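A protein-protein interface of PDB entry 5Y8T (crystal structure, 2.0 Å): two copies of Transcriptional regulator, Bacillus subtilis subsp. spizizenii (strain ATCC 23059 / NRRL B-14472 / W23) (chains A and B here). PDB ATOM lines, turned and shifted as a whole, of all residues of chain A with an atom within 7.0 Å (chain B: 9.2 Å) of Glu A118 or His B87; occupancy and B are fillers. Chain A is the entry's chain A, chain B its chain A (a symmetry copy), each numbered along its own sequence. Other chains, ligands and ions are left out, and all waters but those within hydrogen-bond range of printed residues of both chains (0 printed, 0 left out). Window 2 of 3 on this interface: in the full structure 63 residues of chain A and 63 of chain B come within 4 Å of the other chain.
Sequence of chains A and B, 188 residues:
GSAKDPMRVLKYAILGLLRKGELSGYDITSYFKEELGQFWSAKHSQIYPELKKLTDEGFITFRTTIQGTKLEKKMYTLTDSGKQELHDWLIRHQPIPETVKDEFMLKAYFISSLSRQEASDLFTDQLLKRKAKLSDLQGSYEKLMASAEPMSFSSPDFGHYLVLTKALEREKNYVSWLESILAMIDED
No position is printed for both chains. Of the 9 pairs that touch across the chains among the printed residues, none has its exchanged pair printed and touching as well.
Among the printed residues, merely in contact across the chains: Ser A113 with Arg B19 (3.4 Å), Ser A113 with Leu B90 (3.4 Å), Leu A114 with Leu B90 (3.8 Å), Leu A114 with Ile B91 (3.7 Å), Arg A116 with Phe B153 (3.5 Å), Glu A118 with His B87 (3.2 Å), Ala A119 with Phe B153 (3.9 Å), Asp A121 with His B93 (3.9 Å) and Leu A122 with Leu B90 (3.6 Å).
Of chain A, only Glu A118 comes within 4 Å of His B87. Leu A114 touches just these residues of chain B: Leu B90 and Ile B91. No residue of chain B comes within 4 Å of Ser A115. Printed residues of chain B within 4 Å of Leu A122: Leu B90 (3.6 Å). Of the printed residues of chain A, Phe B153 touches Arg A116 (3.5 Å) and Ala A119 (3.9 Å). Of the printed residues of chain A, Arg B19 touches Ser A113. Of the printed residues of chain A, Leu B90 touches Ser A113 (3.4 Å), Leu A114 (3.8 Å) and Leu A122 (3.6 Å). Printed residues of chain A within 4 Å of Ile B91: Leu A114. The nearest residue of chain B that does not touch Glu A118 is Ile B91 (4.3 Å). The nearest residue of chain A that does not touch His B87 is Ser A113 (4.4 Å).
The side-chain carboxylate (OE1) of Glu A118 lies within hydrogen-bond range of the backbone NH (N) of Ser A115 (2.9 Å). O of Ile A185 lies within hydrogen-bond range of NH1 of Arg A116 (2.9 Å). NE2 of Gln A117 is in hydrogen-bond range of OD1 of Asp A121 (2.7 Å). The guanidinium group of Arg B19 sits close to the backbone carbonyl oxygen of Gly B16, 3.2 Å away.
Of the 13 printed residues of chain A, 7 touch a printed residue of chain B. Hydrophobic or aromatic side chains of chain A within 4 Å of the printed part of chain B: Leu A114, Ala A119 and Leu A122. Printed residues of chain B that touch a printed residue of chain A: Arg B19, His B87, Leu B90, Ile B91, His B93 and Phe B153. Hydrophobic or aromatic side chains of chain B that line the printed part of chain A: His B87, Leu B90, Ile B91, His B93 and Phe B153. Among the printed residues, no Asp or Glu carboxylate lies within 4 Å of a Lys or Arg side-chain nitrogen of the other chain.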
ATOM      1  N   SER A 113      13.533  -9.262   1.698  1.00  0.00           N
ATOM      2  CA  SER A 113      12.513 -10.324   1.694  1.00  0.00           C
ATOM      3  C   SER A 113      11.122  -9.852   2.135  1.00  0.00           C
ATOM      4  O   SER A 113      10.214 -10.662   2.215  1.00  0.00           O
ATOM      5  CB  SER A 113      12.909 -11.456   2.627  1.00  0.00           C
ATOM      6  OG  SER A 113      13.979 -12.196   2.083  1.00  0.00           O
ATOM      7  N   LEU A 114      10.955  -8.567   2.453  1.00  0.00           N
ATOM      8  CA  LEU A 114       9.649  -8.025   2.881  1.00  0.00           C
ATOM      9  C   LEU A 114       9.164  -7.076   1.817  1.00  0.00           C
ATOM     10  O   LEU A 114       9.969  -6.376   1.195  1.00  0.00           O
ATOM     11  CB  LEU A 114       9.747  -7.262   4.199  1.00  0.00           C
ATOM     12  CG  LEU A 114      10.044  -8.093   5.441  1.00  0.00           C
ATOM     13  CD1 LEU A 114      10.266  -7.232   6.692  1.00  0.00           C
ATOM     14  CD2 LEU A 114       8.930  -9.119   5.635  1.00  0.00           C
ATOM     15  N   SER A 115       7.857  -7.062   1.604  1.00  0.00           N
ATOM     16  CA  SER A 115       7.216  -5.999   0.851  1.00  0.00           C
ATOM     17  C   SER A 115       7.331  -4.694   1.600  1.00  0.00           C
ATOM     18  O   SER A 115       7.633  -4.661   2.820  1.00  0.00           O
ATOM     19  CB  SER A 115       5.748  -6.313   0.617  1.00  0.00           C
ATOM     20  OG  SER A 115       5.040  -6.208   1.837  1.00  0.00           O
ATOM     21  N   ARG A 116       7.062  -3.612   0.885  1.00  0.00           N
ATOM     22  CA  ARG A 116       7.137  -2.296   1.468  1.00  0.00           C
ATOM     23  C   ARG A 116       6.127  -2.175   2.574  1.00  0.00           C
ATOM     24  O   ARG A 116       6.407  -1.573   3.624  1.00  0.00           O
ATOM     25  CB  ARG A 116       6.888  -1.224   0.425  1.00  0.00           C
ATOM     26  CG  ARG A 116       7.180   0.181   0.905  1.00  0.00           C
ATOM     27  CD  ARG A 116       6.671   1.250  -0.107  1.00  0.00           C
ATOM     28  NE  ARG A 116       7.517   1.408  -1.286  1.00  0.00           N
ATOM     29  CZ  ARG A 116       8.564   2.240  -1.392  1.00  0.00           C
ATOM     30  NH1 ARG A 116       8.939   2.978  -0.380  1.00  0.00           N
ATOM     31  NH2 ARG A 116       9.239   2.328  -2.539  1.00  0.00           N
ATOM     32  N   GLN A 117       4.939  -2.732   2.352  1.00  0.00           N
ATOM     33  CA  GLN A 117       3.909  -2.730   3.386  1.00  0.00           C
ATOM     34  C   GLN A 117       4.312  -3.569   4.619  1.00  0.00           C
ATOM     35  O   GLN A 117       4.049  -3.159   5.752  1.00  0.00           O
ATOM     36  CB  GLN A 117       2.562  -3.190   2.819  1.00  0.00           C
ATOM     37  CG  GLN A 117       1.447  -3.240   3.842  1.00  0.00           C
ATOM     38  CD  GLN A 117       1.095  -1.858   4.373  1.00  0.00           C
ATOM     39  OE1 GLN A 117       0.666  -0.982   3.604  1.00  0.00           O
ATOM     40  NE2 GLN A 117       1.270  -1.652   5.681  1.00  0.00           N
ATOM     41  N   GLU A 118       4.961  -4.715   4.420  1.00  0.00           N
ATOM     42  CA  GLU A 118       5.353  -5.557   5.560  1.00  0.00           C
ATOM     43  C   GLU A 118       6.482  -4.902   6.341  1.00  0.00           C
ATOM     44  O   GLU A 118       6.537  -4.990   7.566  1.00  0.00           O
ATOM     45  CB  GLU A 118       5.785  -6.944   5.106  1.00  0.00           C
ATOM     46  CG  GLU A 118       4.653  -7.809   4.614  1.00  0.00           C
ATOM     47  CD  GLU A 118       5.119  -8.966   3.753  1.00  0.00           C
ATOM     48  OE1 GLU A 118       6.164  -8.875   3.057  1.00  0.00           O
ATOM     49  OE2 GLU A 118       4.418  -9.994   3.781  1.00  0.00           O
ATOM     50  N   ALA A 119       7.387  -4.256   5.620  1.00  0.00           N
ATOM     51  CA  ALA A 119       8.446  -3.482   6.241  1.00  0.00           C
ATOM     52  C   ALA A 119       7.870  -2.359   7.094  1.00  0.00           C
ATOM     53  O   ALA A 119       8.319  -2.134   8.209  1.00  0.00           O
ATOM     54  CB  ALA A 119       9.386  -2.913   5.186  1.00  0.00           C
ATOM     55  N   SER A 120       6.889  -1.648   6.557  1.00  0.00           N
ATOM     56  CA  SER A 120       6.241  -0.590   7.286  1.00  0.00           C
ATOM     57  C   SER A 120       5.632  -1.144   8.569  1.00  0.00           C
ATOM     58  O   SER A 120       5.890  -0.599   9.648  1.00  0.00           O
ATOM     59  CB  SER A 120       5.175   0.099   6.430  1.00  0.00           C
ATOM     60  OG  SER A 120       4.616   1.181   7.142  1.00  0.00           O
ATOM     61  N   ASP A 121       4.869  -2.232   8.468  1.00  0.00           N
ATOM     62  CA  ASP A 121       4.225  -2.834   9.642  1.00  0.00           C
ATOM     63  C   ASP A 121       5.238  -3.236  10.706  1.00  0.00           C
ATOM     64  O   ASP A 121       5.036  -2.957  11.890  1.00  0.00           O
ATOM     65  CB  ASP A 121       3.346  -4.039   9.259  1.00  0.00           C
ATOM     66  CG  ASP A 121       2.151  -3.652   8.339  1.00  0.00           C
ATOM     67  OD1 ASP A 121       1.802  -2.442   8.229  1.00  0.00           O
ATOM     68  OD2 ASP A 121       1.540  -4.562   7.732  1.00  0.00           O
ATOM     69  N   LEU A 122       6.354  -3.845  10.285  1.00  0.00           N
ATOM     70  CA  LEU A 122       7.373  -4.313  11.221  1.00  0.00           C
ATOM     71  C   LEU A 122       8.076  -3.124  11.918  1.00  0.00           C
ATOM     72  O   LEU A 122       8.258  -3.133  13.122  1.00  0.00           O
ATOM     73  CB  LEU A 122       8.400  -5.177  10.490  1.00  0.00           C
ATOM     74  CG  LEU A 122       9.662  -5.615  11.255  1.00  0.00           C
ATOM     75  CD1 LEU A 122       9.280  -6.620  12.373  1.00  0.00           C
ATOM     76  CD2 LEU A 122      10.710  -6.179  10.276  1.00  0.00           C
ATOM     77  N   PHE A 123       8.442  -2.110  11.153  1.00  0.00           N
ATOM     78  CA  PHE A 123       9.106  -0.952  11.703  1.00  0.00           C
ATOM     79  C   PHE A 123       8.191  -0.128  12.584  1.00  0.00           C
ATOM     80  O   PHE A 123       8.665   0.425  13.571  1.00  0.00           O
ATOM     81  CB  PHE A 123       9.724  -0.116  10.632  1.00  0.00           C
ATOM     82  CG  PHE A 123      11.100  -0.606  10.234  1.00  0.00           C
ATOM     83  CD1 PHE A 123      11.253  -1.846   9.681  1.00  0.00           C
ATOM     84  CD2 PHE A 123      12.205   0.134  10.492  1.00  0.00           C
ATOM     85  CE1 PHE A 123      12.538  -2.319   9.311  1.00  0.00           C
ATOM     86  CE2 PHE A 123      13.488  -0.330  10.175  1.00  0.00           C
ATOM     87  CZ  PHE A 123      13.631  -1.552   9.565  1.00  0.00           C
ATOM     88  N   THR A 124       6.910  -0.047  12.214  1.00  0.00           N
ATOM     89  CA  THR A 124       5.932   0.700  13.000  1.00  0.00           C
ATOM     90  C   THR A 124       5.730   0.048  14.364  1.00  0.00           C
ATOM     91  O   THR A 124       5.714   0.750  15.388  1.00  0.00           O
ATOM     92  CB  THR A 124       4.610   0.803  12.275  1.00  0.00           C
ATOM     93  OG1 THR A 124       4.802   1.582  11.097  1.00  0.00           O
ATOM     94  CG2 THR A 124       3.523   1.464  13.149  1.00  0.00           C
ATOM     95  N   ILE A 185      10.630   4.247   4.121  1.00  0.00           N
ATOM     96  CA  ILE A 185       9.755   3.144   3.758  1.00  0.00           C
ATOM     97  C   ILE A 185       8.415   3.675   3.287  1.00  0.00           C
ATOM     98  O   ILE A 185       7.930   3.220   2.286  1.00  0.00           O
ATOM     99  CB  ILE A 185       9.541   2.151   4.882  1.00  0.00           C
ATOM    100  CG1 ILE A 185      10.849   1.420   5.211  1.00  0.00           C
ATOM    101  CG2 ILE A 185       8.416   1.138   4.467  1.00  0.00           C
ATOM    102  CD1 ILE A 185      10.847   0.684   6.536  1.00  0.00           C
ATOM    103  N   TYR B  12      18.196 -18.085  11.797  1.00  0.00           N
ATOM    104  CA  TYR B  12      17.647 -17.097  10.862  1.00  0.00           C
ATOM    105  C   TYR B  12      18.691 -16.291  10.106  1.00  0.00           C
ATOM    106  O   TYR B  12      18.431 -15.858   8.982  1.00  0.00           O
ATOM    107  CB  TYR B  12      16.646 -16.194  11.579  1.00  0.00           C
ATOM    108  CG  TYR B  12      15.425 -17.000  12.019  1.00  0.00           C
ATOM    109  CD1 TYR B  12      14.499 -17.451  11.090  1.00  0.00           C
ATOM    110  CD2 TYR B  12      15.231 -17.357  13.347  1.00  0.00           C
ATOM    111  CE1 TYR B  12      13.400 -18.187  11.471  1.00  0.00           C
ATOM    112  CE2 TYR B  12      14.108 -18.109  13.736  1.00  0.00           C
ATOM    113  CZ  TYR B  12      13.208 -18.501  12.781  1.00  0.00           C
ATOM    114  OH  TYR B  12      12.132 -19.259  13.114  1.00  0.00           O
ATOM    115  N   LEU B  15      19.344 -18.771   7.236  1.00  0.00           N
ATOM    116  CA  LEU B  15      18.214 -18.784   6.308  1.00  0.00           C
ATOM    117  C   LEU B  15      18.172 -17.479   5.506  1.00  0.00           C
ATOM    118  O   LEU B  15      17.930 -17.477   4.303  1.00  0.00           O
ATOM    119  CB  LEU B  15      16.872 -19.024   7.029  1.00  0.00           C
ATOM    120  CG  LEU B  15      16.654 -20.420   7.652  1.00  0.00           C
ATOM    121  CD1 LEU B  15      15.323 -20.452   8.410  1.00  0.00           C
ATOM    122  CD2 LEU B  15      16.678 -21.496   6.635  1.00  0.00           C
ATOM    123  N   GLY B  16      18.422 -16.368   6.185  1.00  0.00           N
ATOM    124  CA  GLY B  16      18.447 -15.071   5.525  1.00  0.00           C
ATOM    125  C   GLY B  16      19.532 -14.955   4.491  1.00  0.00           C
ATOM    126  O   GLY B  16      19.310 -14.423   3.411  1.00  0.00           O
ATOM    127  N   ARG B  19      18.699 -16.254   1.152  1.00  0.00           N
ATOM    128  CA  ARG B  19      17.426 -15.735   0.639  1.00  0.00           C
ATOM    129  C   ARG B  19      17.576 -15.293  -0.795  1.00  0.00           C
ATOM    130  O   ARG B  19      16.592 -15.284  -1.513  1.00  0.00           O
ATOM    131  CB  ARG B  19      16.888 -14.579   1.487  1.00  0.00           C
ATOM    132  CG  ARG B  19      17.540 -13.222   1.213  1.00  0.00           C
ATOM    133  CD  ARG B  19      17.357 -12.244   2.338  1.00  0.00           C
ATOM    134  NE  ARG B  19      17.872 -10.923   1.999  1.00  0.00           N
ATOM    135  CZ  ARG B  19      19.149 -10.581   2.040  1.00  0.00           C
ATOM    136  NH1 ARG B  19      20.089 -11.461   2.401  1.00  0.00           N
ATOM    137  NH2 ARG B  19      19.497  -9.350   1.706  1.00  0.00           N
ATOM    138  N   LEU B  78      17.604 -22.665   0.008  1.00  0.00           N
ATOM    139  CA  LEU B  78      16.380 -22.702   0.793  1.00  0.00           C
ATOM    140  C   LEU B  78      15.375 -23.611   0.117  1.00  0.00           C
ATOM    141  O   LEU B  78      15.260 -23.604  -1.093  1.00  0.00           O
ATOM    142  CB  LEU B  78      15.727 -21.329   0.891  1.00  0.00           C
ATOM    143  CG  LEU B  78      16.216 -20.241   1.823  1.00  0.00           C
ATOM    144  CD1 LEU B  78      15.336 -19.006   1.604  1.00  0.00           C
ATOM    145  CD2 LEU B  78      16.164 -20.667   3.292  1.00  0.00           C
ATOM    146  N   THR B  79      14.635 -24.386   0.897  1.00  0.00           N
ATOM    147  CA  THR B  79      13.467 -25.070   0.382  1.00  0.00           C
ATOM    148  C   THR B  79      12.300 -24.086   0.490  1.00  0.00           C
ATOM    149  O   THR B  79      12.450 -23.010   1.079  1.00  0.00           O
ATOM    150  CB  THR B  79      13.155 -26.341   1.200  1.00  0.00           C
ATOM    151  OG1 THR B  79      12.912 -25.979   2.569  1.00  0.00           O
ATOM    152  CG2 THR B  79      14.315 -27.331   1.127  1.00  0.00           C
ATOM    153  N   ASP B  80      11.149 -24.471  -0.060  1.00  0.00           N
ATOM    154  CA  ASP B  80       9.894 -23.744   0.161  1.00  0.00           C
ATOM    155  C   ASP B  80       9.660 -23.577   1.662  1.00  0.00           C
ATOM    156  O   ASP B  80       9.288 -22.506   2.124  1.00  0.00           O
ATOM    157  CB  ASP B  80       8.706 -24.517  -0.420  1.00  0.00           C
ATOM    158  CG  ASP B  80       8.704 -24.546  -1.933  1.00  0.00           C
ATOM    159  OD1 ASP B  80       9.546 -23.868  -2.553  1.00  0.00           O
ATOM    160  OD2 ASP B  80       7.857 -25.260  -2.500  1.00  0.00           O
ATOM    161  N   SER B  81       9.878 -24.663   2.400  1.00  0.00           N
ATOM    162  CA  SER B  81       9.722 -24.662   3.833  1.00  0.00           C
ATOM    163  C   SER B  81      10.620 -23.632   4.520  1.00  0.00           C
ATOM    164  O   SER B  81      10.177 -22.924   5.424  1.00  0.00           O
ATOM    165  CB  SER B  81      10.055 -26.034   4.396  1.00  0.00           C
ATOM    166  OG  SER B  81       9.578 -26.111   5.715  1.00  0.00           O
ATOM    167  N   GLY B  82      11.880 -23.569   4.103  1.00  0.00           N
ATOM    168  CA  GLY B  82      12.829 -22.590   4.650  1.00  0.00           C
ATOM    169  C   GLY B  82      12.436 -21.152   4.381  1.00  0.00           C
ATOM    170  O   GLY B  82      12.590 -20.283   5.260  1.00  0.00           O
ATOM    171  N   LYS B  83      11.940 -20.901   3.171  1.00  0.00           N
ATOM    172  CA  LYS B  83      11.424 -19.580   2.790  1.00  0.00           C
ATOM    173  C   LYS B  83      10.252 -19.187   3.660  1.00  0.00           C
ATOM    174  O   LYS B  83      10.165 -18.047   4.092  1.00  0.00           O
ATOM    175  CB  LYS B  83      10.979 -19.525   1.320  1.00  0.00           C
ATOM    176  CG  LYS B  83      12.129 -19.404   0.323  1.00  0.00           C
ATOM    177  CD  LYS B  83      11.654 -19.293  -1.146  1.00  0.00           C
ATOM    178  CE  LYS B  83      12.850 -19.447  -2.103  1.00  0.00           C
ATOM    179  NZ  LYS B  83      12.463 -19.362  -3.547  1.00  0.00           N
ATOM    180  N   GLN B  84       9.330 -20.106   3.892  1.00  0.00           N
ATOM    181  CA  GLN B  84       8.190 -19.808   4.747  1.00  0.00           C
ATOM    182  C   GLN B  84       8.647 -19.519   6.173  1.00  0.00           C
ATOM    183  O   GLN B  84       8.191 -18.563   6.772  1.00  0.00           O
ATOM    184  CB  GLN B  84       7.170 -20.956   4.727  1.00  0.00           C
ATOM    185  CG  GLN B  84       5.844 -20.601   5.397  1.00  0.00           C
ATOM    186  CD  GLN B  84       5.037 -19.574   4.576  1.00  0.00           C
ATOM    187  OE1 GLN B  84       4.668 -19.842   3.436  1.00  0.00           O
ATOM    188  NE2 GLN B  84       4.763 -18.401   5.163  1.00  0.00           N
ATOM    189  N   GLU B  85       9.547 -20.354   6.704  1.00  0.00           N
ATOM    190  CA  GLU B  85      10.095 -20.190   8.058  1.00  0.00           C
ATOM    191  C   GLU B  85      10.775 -18.814   8.231  1.00  0.00           C
ATOM    192  O   GLU B  85      10.572 -18.105   9.225  1.00  0.00           O
ATOM    193  CB  GLU B  85      11.078 -21.330   8.327  1.00  0.00           C
ATOM    194  CG  GLU B  85      11.599 -21.470   9.764  1.00  0.00           C
ATOM    195  CD  GLU B  85      10.553 -21.982  10.780  1.00  0.00           C
ATOM    196  OE1 GLU B  85       9.389 -22.243  10.404  1.00  0.00           O
ATOM    197  OE2 GLU B  85      10.917 -22.121  11.973  1.00  0.00           O
ATOM    198  N   LEU B  86      11.580 -18.428   7.255  1.00  0.00           N
ATOM    199  CA  LEU B  86      12.192 -17.098   7.242  1.00  0.00           C
ATOM    200  C   LEU B  86      11.141 -15.984   7.206  1.00  0.00           C
ATOM    201  O   LEU B  86      11.199 -15.029   7.985  1.00  0.00           O
ATOM    202  CB  LEU B  86      13.076 -16.958   6.012  1.00  0.00           C
ATOM    203  CG  LEU B  86      13.819 -15.648   5.776  1.00  0.00           C
ATOM    204  CD1 LEU B  86      14.685 -15.266   6.988  1.00  0.00           C
ATOM    205  CD2 LEU B  86      14.637 -15.747   4.467  1.00  0.00           C
ATOM    206  N   HIS B  87      10.202 -16.100   6.285  1.00  0.00           N
ATOM    207  CA  HIS B  87       9.155 -15.112   6.143  1.00  0.00           C
ATOM    208  C   HIS B  87       8.360 -14.954   7.442  1.00  0.00           C
ATOM    209  O   HIS B  87       8.075 -13.828   7.860  1.00  0.00           O
ATOM    210  CB  HIS B  87       8.192 -15.496   5.022  1.00  0.00           C
ATOM    211  CG  HIS B  87       7.086 -14.520   4.846  1.00  0.00           C
ATOM    212  ND1 HIS B  87       7.292 -13.267   4.317  1.00  0.00           N
ATOM    213  CD2 HIS B  87       5.781 -14.575   5.205  1.00  0.00           C
ATOM    214  CE1 HIS B  87       6.150 -12.602   4.314  1.00  0.00           C
ATOM    215  NE2 HIS B  87       5.216 -13.373   4.845  1.00  0.00           N
ATOM    216  N   ASP B  88       8.014 -16.073   8.078  1.00  0.00           N
ATOM    217  CA  ASP B  88       7.193 -16.042   9.303  1.00  0.00           C
ATOM    218  C   ASP B  88       7.926 -15.316  10.411  1.00  0.00           C
ATOM    219  O   ASP B  88       7.336 -14.556  11.166  1.00  0.00           O
ATOM    220  CB  ASP B  88       6.848 -17.463   9.755  1.00  0.00           C
ATOM    221  CG  ASP B  88       5.827 -18.139   8.844  1.00  0.00           C
ATOM    222  OD1 ASP B  88       5.243 -17.482   7.968  1.00  0.00           O
ATOM    223  OD2 ASP B  88       5.602 -19.342   9.018  1.00  0.00           O
ATOM    224  N   TRP B  89       9.239 -15.539  10.493  1.00  0.00           N
ATOM    225  CA  TRP B  89      10.038 -14.893  11.500  1.00  0.00           C
ATOM    226  C   TRP B  89      10.156 -13.392  11.206  1.00  0.00           C
ATOM    227  O   TRP B  89       9.992 -12.579  12.092  1.00  0.00           O
ATOM    228  CB  TRP B  89      11.400 -15.585  11.569  1.00  0.00           C
ATOM    229  CG  TRP B  89      12.469 -14.823  12.288  1.00  0.00           C
ATOM    230  CD1 TRP B  89      12.654 -14.737  13.637  1.00  0.00           C
ATOM    231  CD2 TRP B  89      13.525 -14.085  11.686  1.00  0.00           C
ATOM    232  NE1 TRP B  89      13.745 -13.960  13.912  1.00  0.00           N
ATOM    233  CE2 TRP B  89      14.313 -13.565  12.729  1.00  0.00           C
ATOM    234  CE3 TRP B  89      13.888 -13.817  10.364  1.00  0.00           C
ATOM    235  CZ2 TRP B  89      15.441 -12.792  12.495  1.00  0.00           C
ATOM    236  CZ3 TRP B  89      15.029 -13.051  10.135  1.00  0.00           C
ATOM    237  CH2 TRP B  89      15.776 -12.542  11.189  1.00  0.00           C
ATOM    238  N   LEU B  90      10.387 -13.050   9.948  1.00  0.00           N
ATOM    239  CA  LEU B  90      10.488 -11.653   9.522  1.00  0.00           C
ATOM    240  C   LEU B  90       9.310 -10.791   9.921  1.00  0.00           C
ATOM    241  O   LEU B  90       9.512  -9.678  10.415  1.00  0.00           O
ATOM    242  CB  LEU B  90      10.704 -11.525   8.011  1.00  0.00           C
ATOM    243  CG  LEU B  90      12.138 -11.781   7.490  1.00  0.00           C
ATOM    244  CD1 LEU B  90      12.132 -11.844   5.939  1.00  0.00           C
ATOM    245  CD2 LEU B  90      13.091 -10.730   8.015  1.00  0.00           C
ATOM    246  N   ILE B  91       8.099 -11.295   9.740  1.00  0.00           N
ATOM    247  CA  ILE B  91       6.915 -10.510  10.038  1.00  0.00           C
ATOM    248  C   ILE B  91       6.426 -10.615  11.503  1.00  0.00           C
ATOM    249  O   ILE B  91       5.553  -9.873  11.911  1.00  0.00           O
ATOM    250  CB  ILE B  91       5.756 -10.827   9.074  1.00  0.00           C
ATOM    251  CG1 ILE B  91       5.190 -12.226   9.330  1.00  0.00           C
ATOM    252  CG2 ILE B  91       6.214 -10.664   7.623  1.00  0.00           C
ATOM    253  CD1 ILE B  91       3.909 -12.535   8.508  1.00  0.00           C
ATOM    254  N   ARG B  92       7.006 -11.520  12.281  1.00  0.00           N
ATOM    255  CA  ARG B  92       6.569 -11.725  13.659  1.00  0.00           C
ATOM    256  C   ARG B  92       6.924 -10.515  14.528  1.00  0.00           C
ATOM    257  O   ARG B  92       8.048 -10.041  14.508  1.00  0.00           O
ATOM    258  CB  ARG B  92       7.207 -12.988  14.245  1.00  0.00           C
ATOM    259  CG  ARG B  92       6.398 -13.673  15.363  1.00  0.00           C
ATOM    260  CD  ARG B  92       6.292 -15.202  15.105  1.00  0.00           C
ATOM    261  NE  ARG B  92       7.630 -15.809  14.997  1.00  0.00           N
ATOM    262  CZ  ARG B  92       7.982 -16.814  14.176  1.00  0.00           C
ATOM    263  NH1 ARG B  92       7.118 -17.390  13.348  1.00  0.00           N
ATOM    264  NH2 ARG B  92       9.232 -17.254  14.189  1.00  0.00           N
ATOM    265  N   HIS B  93       5.944 -10.016  15.264  1.00  0.00           N
ATOM    266  CA  HIS B  93       6.183  -8.924  16.199  1.00  0.00           C
ATOM    267  C   HIS B  93       6.557  -9.606  17.508  1.00  0.00           C
ATOM    268  O   HIS B  93       5.852 -10.493  17.977  1.00  0.00           O
ATOM    269  CB  HIS B  93       4.921  -8.085  16.421  1.00  0.00           C
ATOM    270  CG  HIS B  93       4.403  -7.408  15.193  1.00  0.00           C
ATOM    271  ND1 HIS B  93       3.116  -6.915  15.113  1.00  0.00           N
ATOM    272  CD2 HIS B  93       4.984  -7.151  13.999  1.00  0.00           C
ATOM    273  CE1 HIS B  93       2.925  -6.393  13.912  1.00  0.00           C
ATOM    274  NE2 HIS B  93       4.042  -6.520  13.220  1.00  0.00           N
ATOM    275  N   GLN B  94       7.670  -9.195  18.067  1.00  0.00           N
ATOM    276  CA  GLN B  94       8.266  -9.802  19.258  1.00  0.00           C
ATOM    277  C   GLN B  94       8.435  -8.701  20.293  1.00  0.00           C
ATOM    278  O   GLN B  94       8.657  -7.558  19.921  1.00  0.00           O
ATOM    279  CB  GLN B  94       9.622 -10.432  18.863  1.00  0.00           C
ATOM    280  CG  GLN B  94       9.426 -11.598  17.838  1.00  0.00           C
ATOM    281  CD  GLN B  94      10.705 -12.125  17.147  1.00  0.00           C
ATOM    282  OE1 GLN B  94      10.660 -12.553  15.976  1.00  0.00           O
ATOM    283  NE2 GLN B  94      11.833 -12.120  17.869  1.00  0.00           N
ATOM    284  N   PHE B 153      14.535   2.723  -0.238  1.00  0.00           N
ATOM    285  CA  PHE B 153      13.960   1.436   0.077  1.00  0.00           C
ATOM    286  C   PHE B 153      14.214   0.395  -1.027  1.00  0.00           C
ATOM    287  O   PHE B 153      14.394  -0.779  -0.740  1.00  0.00           O
ATOM    288  CB  PHE B 153      12.450   1.559   0.269  1.00  0.00           C
ATOM    289  CG  PHE B 153      11.783   0.255   0.507  1.00  0.00           C
ATOM    290  CD1 PHE B 153      11.863  -0.354   1.752  1.00  0.00           C
ATOM    291  CD2 PHE B 153      11.095  -0.403  -0.514  1.00  0.00           C
ATOM    292  CE1 PHE B 153      11.259  -1.582   1.982  1.00  0.00           C
ATOM    293  CE2 PHE B 153      10.496  -1.619  -0.271  1.00  0.00           C
ATOM    294  CZ  PHE B 153      10.576  -2.203   0.991  1.00  0.00           C
